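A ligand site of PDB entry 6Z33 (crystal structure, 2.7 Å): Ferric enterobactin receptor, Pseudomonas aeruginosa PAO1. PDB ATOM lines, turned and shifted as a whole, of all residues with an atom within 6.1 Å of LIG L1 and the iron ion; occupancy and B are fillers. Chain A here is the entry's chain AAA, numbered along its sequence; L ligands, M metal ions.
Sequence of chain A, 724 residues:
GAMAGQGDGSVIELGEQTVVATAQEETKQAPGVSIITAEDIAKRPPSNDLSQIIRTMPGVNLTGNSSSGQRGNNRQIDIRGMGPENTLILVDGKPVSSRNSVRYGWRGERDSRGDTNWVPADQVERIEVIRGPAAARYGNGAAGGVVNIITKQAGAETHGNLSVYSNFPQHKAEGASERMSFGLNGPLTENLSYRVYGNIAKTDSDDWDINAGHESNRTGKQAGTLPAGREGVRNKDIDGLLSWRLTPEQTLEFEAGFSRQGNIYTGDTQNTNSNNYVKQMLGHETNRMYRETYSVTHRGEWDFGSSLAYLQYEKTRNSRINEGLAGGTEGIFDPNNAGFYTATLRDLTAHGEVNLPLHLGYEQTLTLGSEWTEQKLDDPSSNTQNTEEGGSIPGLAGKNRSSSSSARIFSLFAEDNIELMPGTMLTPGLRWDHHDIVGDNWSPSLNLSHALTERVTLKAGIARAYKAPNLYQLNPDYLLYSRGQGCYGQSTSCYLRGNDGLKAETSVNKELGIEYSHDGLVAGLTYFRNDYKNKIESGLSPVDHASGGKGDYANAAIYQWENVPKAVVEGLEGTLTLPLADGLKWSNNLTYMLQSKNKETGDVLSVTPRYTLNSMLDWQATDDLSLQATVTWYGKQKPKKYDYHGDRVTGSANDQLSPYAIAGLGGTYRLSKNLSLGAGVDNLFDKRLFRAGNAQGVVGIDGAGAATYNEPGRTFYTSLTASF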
ATOM      1  N   GLN A  70      -8.703 -20.860 -10.708  1.00  0.00           N
ATOM      2  CA  GLN A  70      -9.335 -19.559 -11.085  1.00  0.00           C
ATOM      3  C   GLN A  70      -8.819 -18.476 -10.162  1.00  0.00           C
ATOM      4  O   GLN A  70      -8.749 -18.708  -8.967  1.00  0.00           O
ATOM      5  CB  GLN A  70     -10.868 -19.680 -11.025  1.00  0.00           C
ATOM      6  CG  GLN A  70     -11.451 -20.348 -12.265  1.00  0.00           C
ATOM      7  CD  GLN A  70     -12.812 -20.954 -12.089  1.00  0.00           C
ATOM      8  OE1 GLN A  70     -13.145 -21.952 -12.730  1.00  0.00           O
ATOM      9  NE2 GLN A  70     -13.670 -20.278 -11.346  1.00  0.00           N
ATOM     10  N   ARG A 107     -16.738 -22.074  -8.301  1.00  0.00           N
ATOM     11  CA  ARG A 107     -15.591 -22.920  -7.854  1.00  0.00           C
ATOM     12  C   ARG A 107     -15.003 -22.360  -6.559  1.00  0.00           C
ATOM     13  O   ARG A 107     -13.831 -22.726  -6.249  1.00  0.00           O
ATOM     14  CB  ARG A 107     -14.505 -22.962  -8.933  1.00  0.00           C
ATOM     15  CG  ARG A 107     -15.024 -23.200 -10.329  1.00  0.00           C
ATOM     16  CD  ARG A 107     -15.898 -24.423 -10.349  1.00  0.00           C
ATOM     17  NE  ARG A 107     -16.712 -24.582 -11.543  1.00  0.00           N
ATOM     18  CZ  ARG A 107     -17.471 -25.638 -11.757  1.00  0.00           C
ATOM     19  NH1 ARG A 107     -17.456 -26.611 -10.852  1.00  0.00           N
ATOM     20  NH2 ARG A 107     -18.202 -25.751 -12.859  1.00  0.00           N
ATOM     21  N   LYS A 221     -11.157 -20.562 -31.178  1.00  0.00           N
ATOM     22  CA  LYS A 221     -11.632 -19.245 -30.685  1.00  0.00           C
ATOM     23  C   LYS A 221     -10.654 -18.705 -29.626  1.00  0.00           C
ATOM     24  O   LYS A 221     -10.524 -17.463 -29.551  1.00  0.00           O
ATOM     25  CB  LYS A 221     -13.046 -19.350 -30.129  1.00  0.00           C
ATOM     26  CG  LYS A 221     -14.135 -19.406 -31.199  1.00  0.00           C
ATOM     27  CD  LYS A 221     -15.449 -19.953 -30.700  1.00  0.00           C
ATOM     28  CE  LYS A 221     -16.358 -20.442 -31.813  1.00  0.00           C
ATOM     29  NZ  LYS A 221     -17.507 -21.199 -31.269  1.00  0.00           N
ATOM     30  N   GLN A 222      -9.977 -19.572 -28.863  1.00  0.00           N
ATOM     31  CA  GLN A 222      -9.213 -19.130 -27.667  1.00  0.00           C
ATOM     32  C   GLN A 222      -7.729 -18.920 -28.027  1.00  0.00           C
ATOM     33  O   GLN A 222      -6.923 -18.608 -27.128  1.00  0.00           O
ATOM     34  CB  GLN A 222      -9.358 -20.131 -26.502  1.00  0.00           C
ATOM     35  CG  GLN A 222     -10.798 -20.383 -26.067  1.00  0.00           C
ATOM     36  CD  GLN A 222     -11.639 -19.125 -25.920  1.00  0.00           C
ATOM     37  OE1 GLN A 222     -11.165 -18.075 -25.464  1.00  0.00           O
ATOM     38  NE2 GLN A 222     -12.913 -19.256 -26.244  1.00  0.00           N
ATOM     39  N   GLN A 270     -11.653 -15.180 -15.076  1.00  0.00           N
ATOM     40  CA  GLN A 270     -11.917 -16.491 -14.425  1.00  0.00           C
ATOM     41  C   GLN A 270     -11.324 -17.640 -15.256  1.00  0.00           C
ATOM     42  O   GLN A 270     -10.608 -18.473 -14.673  1.00  0.00           O
ATOM     43  CB  GLN A 270     -13.400 -16.704 -14.166  1.00  0.00           C
ATOM     44  CG  GLN A 270     -13.703 -18.057 -13.535  1.00  0.00           C
ATOM     45  CD  GLN A 270     -15.164 -18.219 -13.201  1.00  0.00           C
ATOM     46  OE1 GLN A 270     -15.890 -18.961 -13.860  1.00  0.00           O
ATOM     47  NE2 GLN A 270     -15.630 -17.472 -12.223  1.00  0.00           N
ATOM     48  N   ASN A 271     -11.607 -17.714 -16.558  1.00  0.00           N
ATOM     49  CA  ASN A 271     -11.254 -18.930 -17.329  1.00  0.00           C
ATOM     50  C   ASN A 271     -10.016 -18.677 -18.197  1.00  0.00           C
ATOM     51  O   ASN A 271      -9.634 -19.609 -18.924  1.00  0.00           O
ATOM     52  CB  ASN A 271     -12.447 -19.404 -18.150  1.00  0.00           C
ATOM     53  CG  ASN A 271     -13.690 -19.469 -17.305  1.00  0.00           C
ATOM     54  OD1 ASN A 271     -14.578 -18.628 -17.437  1.00  0.00           O
ATOM     55  ND2 ASN A 271     -13.627 -20.290 -16.267  1.00  0.00           N
ATOM     56  N   ASN A 273      -9.987 -16.862 -20.747  1.00  0.00           N
ATOM     57  CA  ASN A 273     -10.566 -16.380 -22.031  1.00  0.00           C
ATOM     58  C   ASN A 273     -10.407 -14.861 -22.098  1.00  0.00           C
ATOM     59  O   ASN A 273     -10.115 -14.253 -21.068  1.00  0.00           O
ATOM     60  CB  ASN A 273     -12.035 -16.796 -22.178  1.00  0.00           C
ATOM     61  CG  ASN A 273     -12.904 -16.374 -21.010  1.00  0.00           C
ATOM     62  OD1 ASN A 273     -12.499 -16.457 -19.845  1.00  0.00           O
ATOM     63  ND2 ASN A 273     -14.163 -16.075 -21.298  1.00  0.00           N
ATOM     64  N   ALA A 326     -22.313 -16.584 -16.638  1.00  0.00           N
ATOM     65  CA  ALA A 326     -22.654 -17.835 -17.378  1.00  0.00           C
ATOM     66  C   ALA A 326     -21.404 -18.461 -18.014  1.00  0.00           C
ATOM     67  O   ALA A 326     -20.892 -17.889 -19.000  1.00  0.00           O
ATOM     68  CB  ALA A 326     -23.722 -17.555 -18.414  1.00  0.00           C
ATOM     69  N   GLY A 327     -21.086 -19.685 -17.590  1.00  0.00           N
ATOM     70  CA  GLY A 327     -20.131 -20.589 -18.263  1.00  0.00           C
ATOM     71  C   GLY A 327     -18.750 -19.948 -18.393  1.00  0.00           C
ATOM     72  O   GLY A 327     -18.189 -19.537 -17.370  1.00  0.00           O
ATOM     73  N   GLY A 328     -18.213 -19.933 -19.611  1.00  0.00           N
ATOM     74  CA  GLY A 328     -16.952 -19.248 -19.938  1.00  0.00           C
ATOM     75  C   GLY A 328     -17.067 -17.732 -19.861  1.00  0.00           C
ATOM     76  O   GLY A 328     -16.020 -17.075 -19.924  1.00  0.00           O
ATOM     77  N   THR A 329     -18.271 -17.182 -19.731  1.00  0.00           N
ATOM     78  CA  THR A 329     -18.445 -15.714 -19.556  1.00  0.00           C
ATOM     79  C   THR A 329     -18.488 -15.341 -18.067  1.00  0.00           C
ATOM     80  O   THR A 329     -18.618 -14.126 -17.765  1.00  0.00           O
ATOM     81  CB  THR A 329     -19.675 -15.167 -20.301  1.00  0.00           C
ATOM     82  OG1 THR A 329     -20.822 -15.457 -19.515  1.00  0.00           O
ATOM     83  CG2 THR A 329     -19.807 -15.738 -21.684  1.00  0.00           C
ATOM     84  N   GLU A 330     -18.470 -16.338 -17.175  1.00  0.00           N
ATOM     85  CA  GLU A 330     -18.380 -16.099 -15.714  1.00  0.00           C
ATOM     86  C   GLU A 330     -16.995 -15.496 -15.418  1.00  0.00           C
ATOM     87  O   GLU A 330     -15.987 -16.133 -15.796  1.00  0.00           O
ATOM     88  CB  GLU A 330     -18.606 -17.415 -14.955  1.00  0.00           C
ATOM     89  CG  GLU A 330     -18.776 -17.235 -13.454  1.00  0.00           C
ATOM     90  CD  GLU A 330     -18.636 -18.533 -12.671  1.00  0.00           C
ATOM     91  OE1 GLU A 330     -18.564 -19.612 -13.320  1.00  0.00           O
ATOM     92  OE2 GLU A 330     -18.518 -18.470 -11.436  1.00  0.00           O
ATOM     93  N   GLU A 389     -32.509 -18.811 -21.707  1.00  0.00           N
ATOM     94  CA  GLU A 389     -31.815 -19.869 -22.480  1.00  0.00           C
ATOM     95  C   GLU A 389     -32.039 -21.251 -21.826  1.00  0.00           C
ATOM     96  O   GLU A 389     -32.480 -22.151 -22.548  1.00  0.00           O
ATOM     97  CB  GLU A 389     -30.332 -19.566 -22.635  1.00  0.00           C
ATOM     98  CG  GLU A 389     -29.736 -20.218 -23.866  1.00  0.00           C
ATOM     99  CD  GLU A 389     -28.279 -19.915 -24.135  1.00  0.00           C
ATOM    100  OE1 GLU A 389     -28.016 -19.107 -25.032  1.00  0.00           O
ATOM    101  OE2 GLU A 389     -27.415 -20.558 -23.510  1.00  0.00           O
ATOM    102  N   TYR A 481     -25.061 -20.019 -14.598  1.00  0.00           N
ATOM    103  CA  TYR A 481     -25.529 -20.880 -15.708  1.00  0.00           C
ATOM    104  C   TYR A 481     -24.310 -21.373 -16.514  1.00  0.00           C
ATOM    105  O   TYR A 481     -23.310 -20.616 -16.669  1.00  0.00           O
ATOM    106  CB  TYR A 481     -26.527 -20.114 -16.578  1.00  0.00           C
ATOM    107  CG  TYR A 481     -26.876 -20.748 -17.905  1.00  0.00           C
ATOM    108  CD1 TYR A 481     -27.742 -21.825 -17.958  1.00  0.00           C
ATOM    109  CD2 TYR A 481     -26.495 -20.165 -19.103  1.00  0.00           C
ATOM    110  CE1 TYR A 481     -28.161 -22.344 -19.181  1.00  0.00           C
ATOM    111  CE2 TYR A 481     -26.908 -20.668 -20.325  1.00  0.00           C
ATOM    112  CZ  TYR A 481     -27.725 -21.782 -20.360  1.00  0.00           C
ATOM    113  OH  TYR A 481     -28.097 -22.350 -21.558  1.00  0.00           O
ATOM    114  N   SER A 482     -24.389 -22.618 -16.961  1.00  0.00           N
ATOM    115  CA  SER A 482     -23.457 -23.222 -17.938  1.00  0.00           C
ATOM    116  C   SER A 482     -24.277 -24.012 -18.951  1.00  0.00           C
ATOM    117  O   SER A 482     -25.319 -24.575 -18.560  1.00  0.00           O
ATOM    118  CB  SER A 482     -22.434 -24.090 -17.269  1.00  0.00           C
ATOM    119  OG  SER A 482     -21.817 -24.961 -18.214  1.00  0.00           O
ATOM    120  N   ARG A 483     -23.808 -24.057 -20.186  1.00  0.00           N
ATOM    121  CA  ARG A 483     -24.400 -24.854 -21.286  1.00  0.00           C
ATOM    122  C   ARG A 483     -23.984 -26.328 -21.151  1.00  0.00           C
ATOM    123  O   ARG A 483     -24.375 -27.125 -22.033  1.00  0.00           O
ATOM    124  CB  ARG A 483     -23.946 -24.282 -22.621  1.00  0.00           C
ATOM    125  CG  ARG A 483     -24.447 -22.872 -22.877  1.00  0.00           C
ATOM    126  CD  ARG A 483     -23.766 -22.179 -24.038  1.00  0.00           C
ATOM    127  NE  ARG A 483     -24.608 -21.122 -24.596  1.00  0.00           N
ATOM    128  CZ  ARG A 483     -24.152 -20.111 -25.343  1.00  0.00           C
ATOM    129  NH1 ARG A 483     -22.859 -20.019 -25.633  1.00  0.00           N
ATOM    130  NH2 ARG A 483     -25.007 -19.206 -25.811  1.00  0.00           N
ATOM    131  N   GLY A 484     -23.112 -26.644 -20.200  1.00  0.00           N
ATOM    132  CA  GLY A 484     -22.712 -28.047 -19.941  1.00  0.00           C
ATOM    133  C   GLY A 484     -21.352 -28.152 -19.333  1.00  0.00           C
ATOM    134  O   GLY A 484     -21.209 -28.916 -18.348  1.00  0.00           O
ATOM    135  N   GLN A 485     -20.368 -27.409 -19.878  1.00  0.00           N
ATOM    136  CA  GLN A 485     -18.907 -27.615 -19.629  1.00  0.00           C
ATOM    137  C   GLN A 485     -18.634 -27.647 -18.124  1.00  0.00           C
ATOM    138  O   GLN A 485     -17.637 -28.295 -17.713  1.00  0.00           O
ATOM    139  CB  GLN A 485     -18.085 -26.484 -20.256  1.00  0.00           C
ATOM    140  CG  GLN A 485     -16.578 -26.678 -20.129  1.00  0.00           C
ATOM    141  CD  GLN A 485     -15.860 -26.407 -21.424  1.00  0.00           C
ATOM    142  OE1 GLN A 485     -14.897 -27.083 -21.781  1.00  0.00           O
ATOM    143  NE2 GLN A 485     -16.382 -25.461 -22.191  1.00  0.00           N
ATOM    144  N   GLY A 486     -19.471 -26.961 -17.334  1.00  0.00           N
ATOM    145  CA  GLY A 486     -19.303 -26.756 -15.886  1.00  0.00           C
ATOM    146  C   GLY A 486     -20.313 -27.529 -15.042  1.00  0.00           C
ATOM    147  O   GLY A 486     -20.390 -27.258 -13.822  1.00  0.00           O
ATOM    148  N   TYR A 644     -14.938 -30.367 -13.900  1.00  0.00           N
ATOM    149  CA  TYR A 644     -16.225 -29.840 -13.418  1.00  0.00           C
ATOM    150  C   TYR A 644     -17.299 -30.910 -13.610  1.00  0.00           C
ATOM    151  O   TYR A 644     -18.409 -30.739 -13.059  1.00  0.00           O
ATOM    152  CB  TYR A 644     -16.571 -28.523 -14.131  1.00  0.00           C
ATOM    153  CG  TYR A 644     -15.484 -27.471 -14.102  1.00  0.00           C
ATOM    154  CD1 TYR A 644     -14.852 -27.109 -12.927  1.00  0.00           C
ATOM    155  CD2 TYR A 644     -15.134 -26.780 -15.252  1.00  0.00           C
ATOM    156  CE1 TYR A 644     -13.842 -26.158 -12.901  1.00  0.00           C
ATOM    157  CE2 TYR A 644     -14.113 -25.838 -15.252  1.00  0.00           C
ATOM    158  CZ  TYR A 644     -13.465 -25.525 -14.072  1.00  0.00           C
ATOM    159  OH  TYR A 644     -12.553 -24.507 -14.052  1.00  0.00           O
ATOM    160  N   VAL A 698     -10.537 -26.771 -20.700  1.00  0.00           N
ATOM    161  CA  VAL A 698     -11.841 -26.428 -21.343  1.00  0.00           C
ATOM    162  C   VAL A 698     -11.630 -26.450 -22.865  1.00  0.00           C
ATOM    163  O   VAL A 698     -10.457 -26.561 -23.306  1.00  0.00           O
ATOM    164  CB  VAL A 698     -12.377 -25.057 -20.870  1.00  0.00           C
ATOM    165  CG1 VAL A 698     -12.837 -25.106 -19.435  1.00  0.00           C
ATOM    166  CG2 VAL A 698     -11.364 -23.946 -21.073  1.00  0.00           C
ATOM    167  N   VAL A 699     -12.707 -26.254 -23.633  1.00  0.00           N
ATOM    168  CA  VAL A 699     -12.659 -26.187 -25.123  1.00  0.00           C
ATOM    169  C   VAL A 699     -11.756 -25.017 -25.550  1.00  0.00           C
ATOM    170  O   VAL A 699     -12.118 -23.859 -25.238  1.00  0.00           O
ATOM    171  CB  VAL A 699     -14.070 -26.051 -25.706  1.00  0.00           C
ATOM    172  CG1 VAL A 699     -14.034 -25.899 -27.224  1.00  0.00           C
ATOM    173  CG2 VAL A 699     -14.959 -27.213 -25.292  1.00  0.00           C
ATOM    174  N   ILE A 701      -8.850 -24.066 -24.475  1.00  0.00           N
ATOM    175  CA  ILE A 701      -7.855 -23.723 -23.420  1.00  0.00           C
ATOM    176  C   ILE A 701      -7.488 -24.976 -22.626  1.00  0.00           C
ATOM    177  O   ILE A 701      -8.188 -25.275 -21.656  1.00  0.00           O
ATOM    178  CB  ILE A 701      -8.350 -22.602 -22.490  1.00  0.00           C
ATOM    179  CG1 ILE A 701      -9.173 -21.552 -23.245  1.00  0.00           C
ATOM    180  CG2 ILE A 701      -7.176 -21.983 -21.751  1.00  0.00           C
ATOM    181  CD1 ILE A 701      -9.760 -20.475 -22.353  1.00  0.00           C
HETATM  182  C1  LIG L   1     -18.124 -18.735 -25.500  1.00  0.00           C
HETATM  183  C2  LIG L   1     -18.167 -23.368 -17.531  1.00  0.00           C
HETATM  184  C3  LIG L   1     -17.990 -18.284 -24.040  1.00  0.00           C
HETATM  185  C4  LIG L   1     -16.608 -18.623 -23.469  1.00  0.00           C
HETATM  186  C5  LIG L   1     -16.118 -22.552 -19.257  1.00  0.00           C
HETATM  187  C6  LIG L   1     -16.413 -20.112 -23.187  1.00  0.00           C
HETATM  188  C7  LIG L   1     -15.020 -20.609 -23.478  1.00  0.00           C
HETATM  189  C8  LIG L   1     -14.324 -21.273 -22.301  1.00  0.00           C
HETATM  190  C9  LIG L   1     -14.999 -22.168 -20.167  1.00  0.00           C
HETATM  191  C10 LIG L   1     -15.928 -22.599 -17.875  1.00  0.00           C
HETATM  192  C11 LIG L   1     -16.929 -22.988 -17.029  1.00  0.00           C
HETATM  193  N1  LIG L   1     -19.135 -19.536 -25.799  1.00  0.00           N
HETATM  194  N2  LIG L   1     -15.216 -22.065 -21.463  1.00  0.00           N
HETATM  195  C12 LIG L   1     -18.982 -20.784 -26.542  1.00  0.00           C
HETATM  196  N3  LIG L   1     -19.052 -18.924 -23.290  1.00  0.00           N
HETATM  197  C13 LIG L   1     -16.656 -20.864 -27.822  1.00  0.00           C
HETATM  198  C14 LIG L   1     -17.702 -20.846 -27.274  1.00  0.00           C
HETATM  199  O1  LIG L   1     -17.303 -18.355 -26.328  1.00  0.00           O
HETATM  200  O2  LIG L   1     -13.906 -21.889 -19.681  1.00  0.00           O
HETATM  201  C15 LIG L   1     -18.401 -23.311 -18.893  1.00  0.00           C
HETATM  202  O3  LIG L   1     -19.632 -23.614 -19.404  1.00  0.00           O
HETATM  203  C16 LIG L   1     -17.380 -22.911 -19.757  1.00  0.00           C
HETATM  204  O4  LIG L   1     -17.681 -22.843 -21.074  1.00  0.00           O
HETATM  205  C17 LIG L   1     -20.321 -18.516 -23.389  1.00  0.00           C
HETATM  206  O5  LIG L   1     -20.641 -17.525 -24.042  1.00  0.00           O
HETATM  207  C18 LIG L   1     -21.337 -19.279 -22.611  1.00  0.00           C
HETATM  208  C19 LIG L   1     -22.665 -18.850 -22.485  1.00  0.00           C
HETATM  209  C20 LIG L   1     -23.568 -19.566 -21.745  1.00  0.00           C
HETATM  210  C21 LIG L   1     -23.170 -20.734 -21.078  1.00  0.00           C
HETATM  211  C22 LIG L   1     -21.859 -21.170 -21.179  1.00  0.00           C
HETATM  212  O6  LIG L   1     -21.453 -22.315 -20.555  1.00  0.00           O
HETATM  213  C23 LIG L   1     -20.938 -20.442 -21.923  1.00  0.00           C
HETATM  214  O7  LIG L   1     -19.698 -20.950 -22.019  1.00  0.00           O
HETATM  215  C1  LG2 L   2     -20.406 -25.576 -22.858  1.00  0.00           C
HETATM  216  O1  LG2 L   2     -20.258 -24.952 -21.589  1.00  0.00           O
HETATM  217  C2  LG2 L   2     -19.933 -24.752 -23.998  1.00  0.00           C
HETATM  218  O2  LG2 L   2     -19.853 -23.362 -23.708  1.00  0.00           O
HETATM  219 FE    FE M   1     -19.737 -22.823 -21.419  1.00  0.00          FE
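OG of Ser 482 lies close to O3 of LIG L1, 2.8 Å away. The backbone NH of Arg 483 sits close to an oxygen (O6) of LIG L1. N of Gly 328 lies close to O7 of LIG L1, at 3.0 Å. NE2 of Gln 485 sits close to O4 of LIG L1.
The backbone NH of Gly 486 sits at hydrogen-bond distance from the side-chain hydroxyl of Ser 482, 3.2 Å away. OG of Ser 482 lies within hydrogen-bond range of N of Gly 484 (2.9 Å). OE2 of Glu 389 lies within salt-bridge range of NE of Arg 483. The backbone carbonyl oxygen of Gly 328 sits close to the side-chain amide oxygen of Asn 271, 3.3 Å away. The backbone carbonyl oxygen of Gly 328 sits at hydrogen-bond distance from the side-chain amide nitrogen of Asn 273. OG1 of Thr 329 sits at hydrogen-bond distance from O of Ala 326 (2.5 Å). OE1 of Gln 485 lies within hydrogen-bond range of N of Val 699 (3.0 Å). N of Gly 327 lies within hydrogen-bond range of O of Tyr 481 (2.6 Å).
Lys 221 touches LIG L1 (CD to C13, 3.3 Å). Gln 222 touches LIG L1. CB of Asn 271 touches O2 of LIG L1, 3.3 Å away. O of Ala 326 touches C23 of LIG L1, at 3.9 Å. Gly 327 touches LIG L1 (CA to O6, 3.2 Å). CG2 of Thr 329 touches O5 of LIG L1, at 3.1 Å. CE2 of Tyr 481 touches C20 of LIG L1, 3.8 Å away. Gly 486 touches LIG L1 (N to C2, 3.8 Å). Val 698 touches LIG L1. Hydrophobic or aromatic side chains that line LIG L1: Ala 326, Tyr 481 and Val 698. Within 4 Å of LIG L1: Lys 221, Gln 222, Asn 271, Ala 326, Gly 327, Gly 328, Thr 329, Tyr 481, Ser 482, Arg 483, Gln 485, Gly 486 and Val 698. The nearest printed residue that does not touch LIG L1 is Asn 273 (4.1 Å).
Gly 327 touches the iron ion. N of Gly 328 touches the iron ion, 3.7 Å away. Along chain A the residues within 4 Å of the iron ion span positions 327 to 328. The nearest printed residue that does not touch the iron ion is Gln 485 (4.2 Å).
O7 of LIG L1 binds the iron ion (2.0 Å). The iron ion is bound by O6 of LIG L1, at 2.0 Å. O4 of LIG L1 binds the iron ion. O3 of LIG L1 is bound to the iron ion, 2.2 Å away. O1 of LG2 L2 is bound to the iron ion, 2.2 Å away. O2 of LG2 L2 binds the iron ion (2.4 Å).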
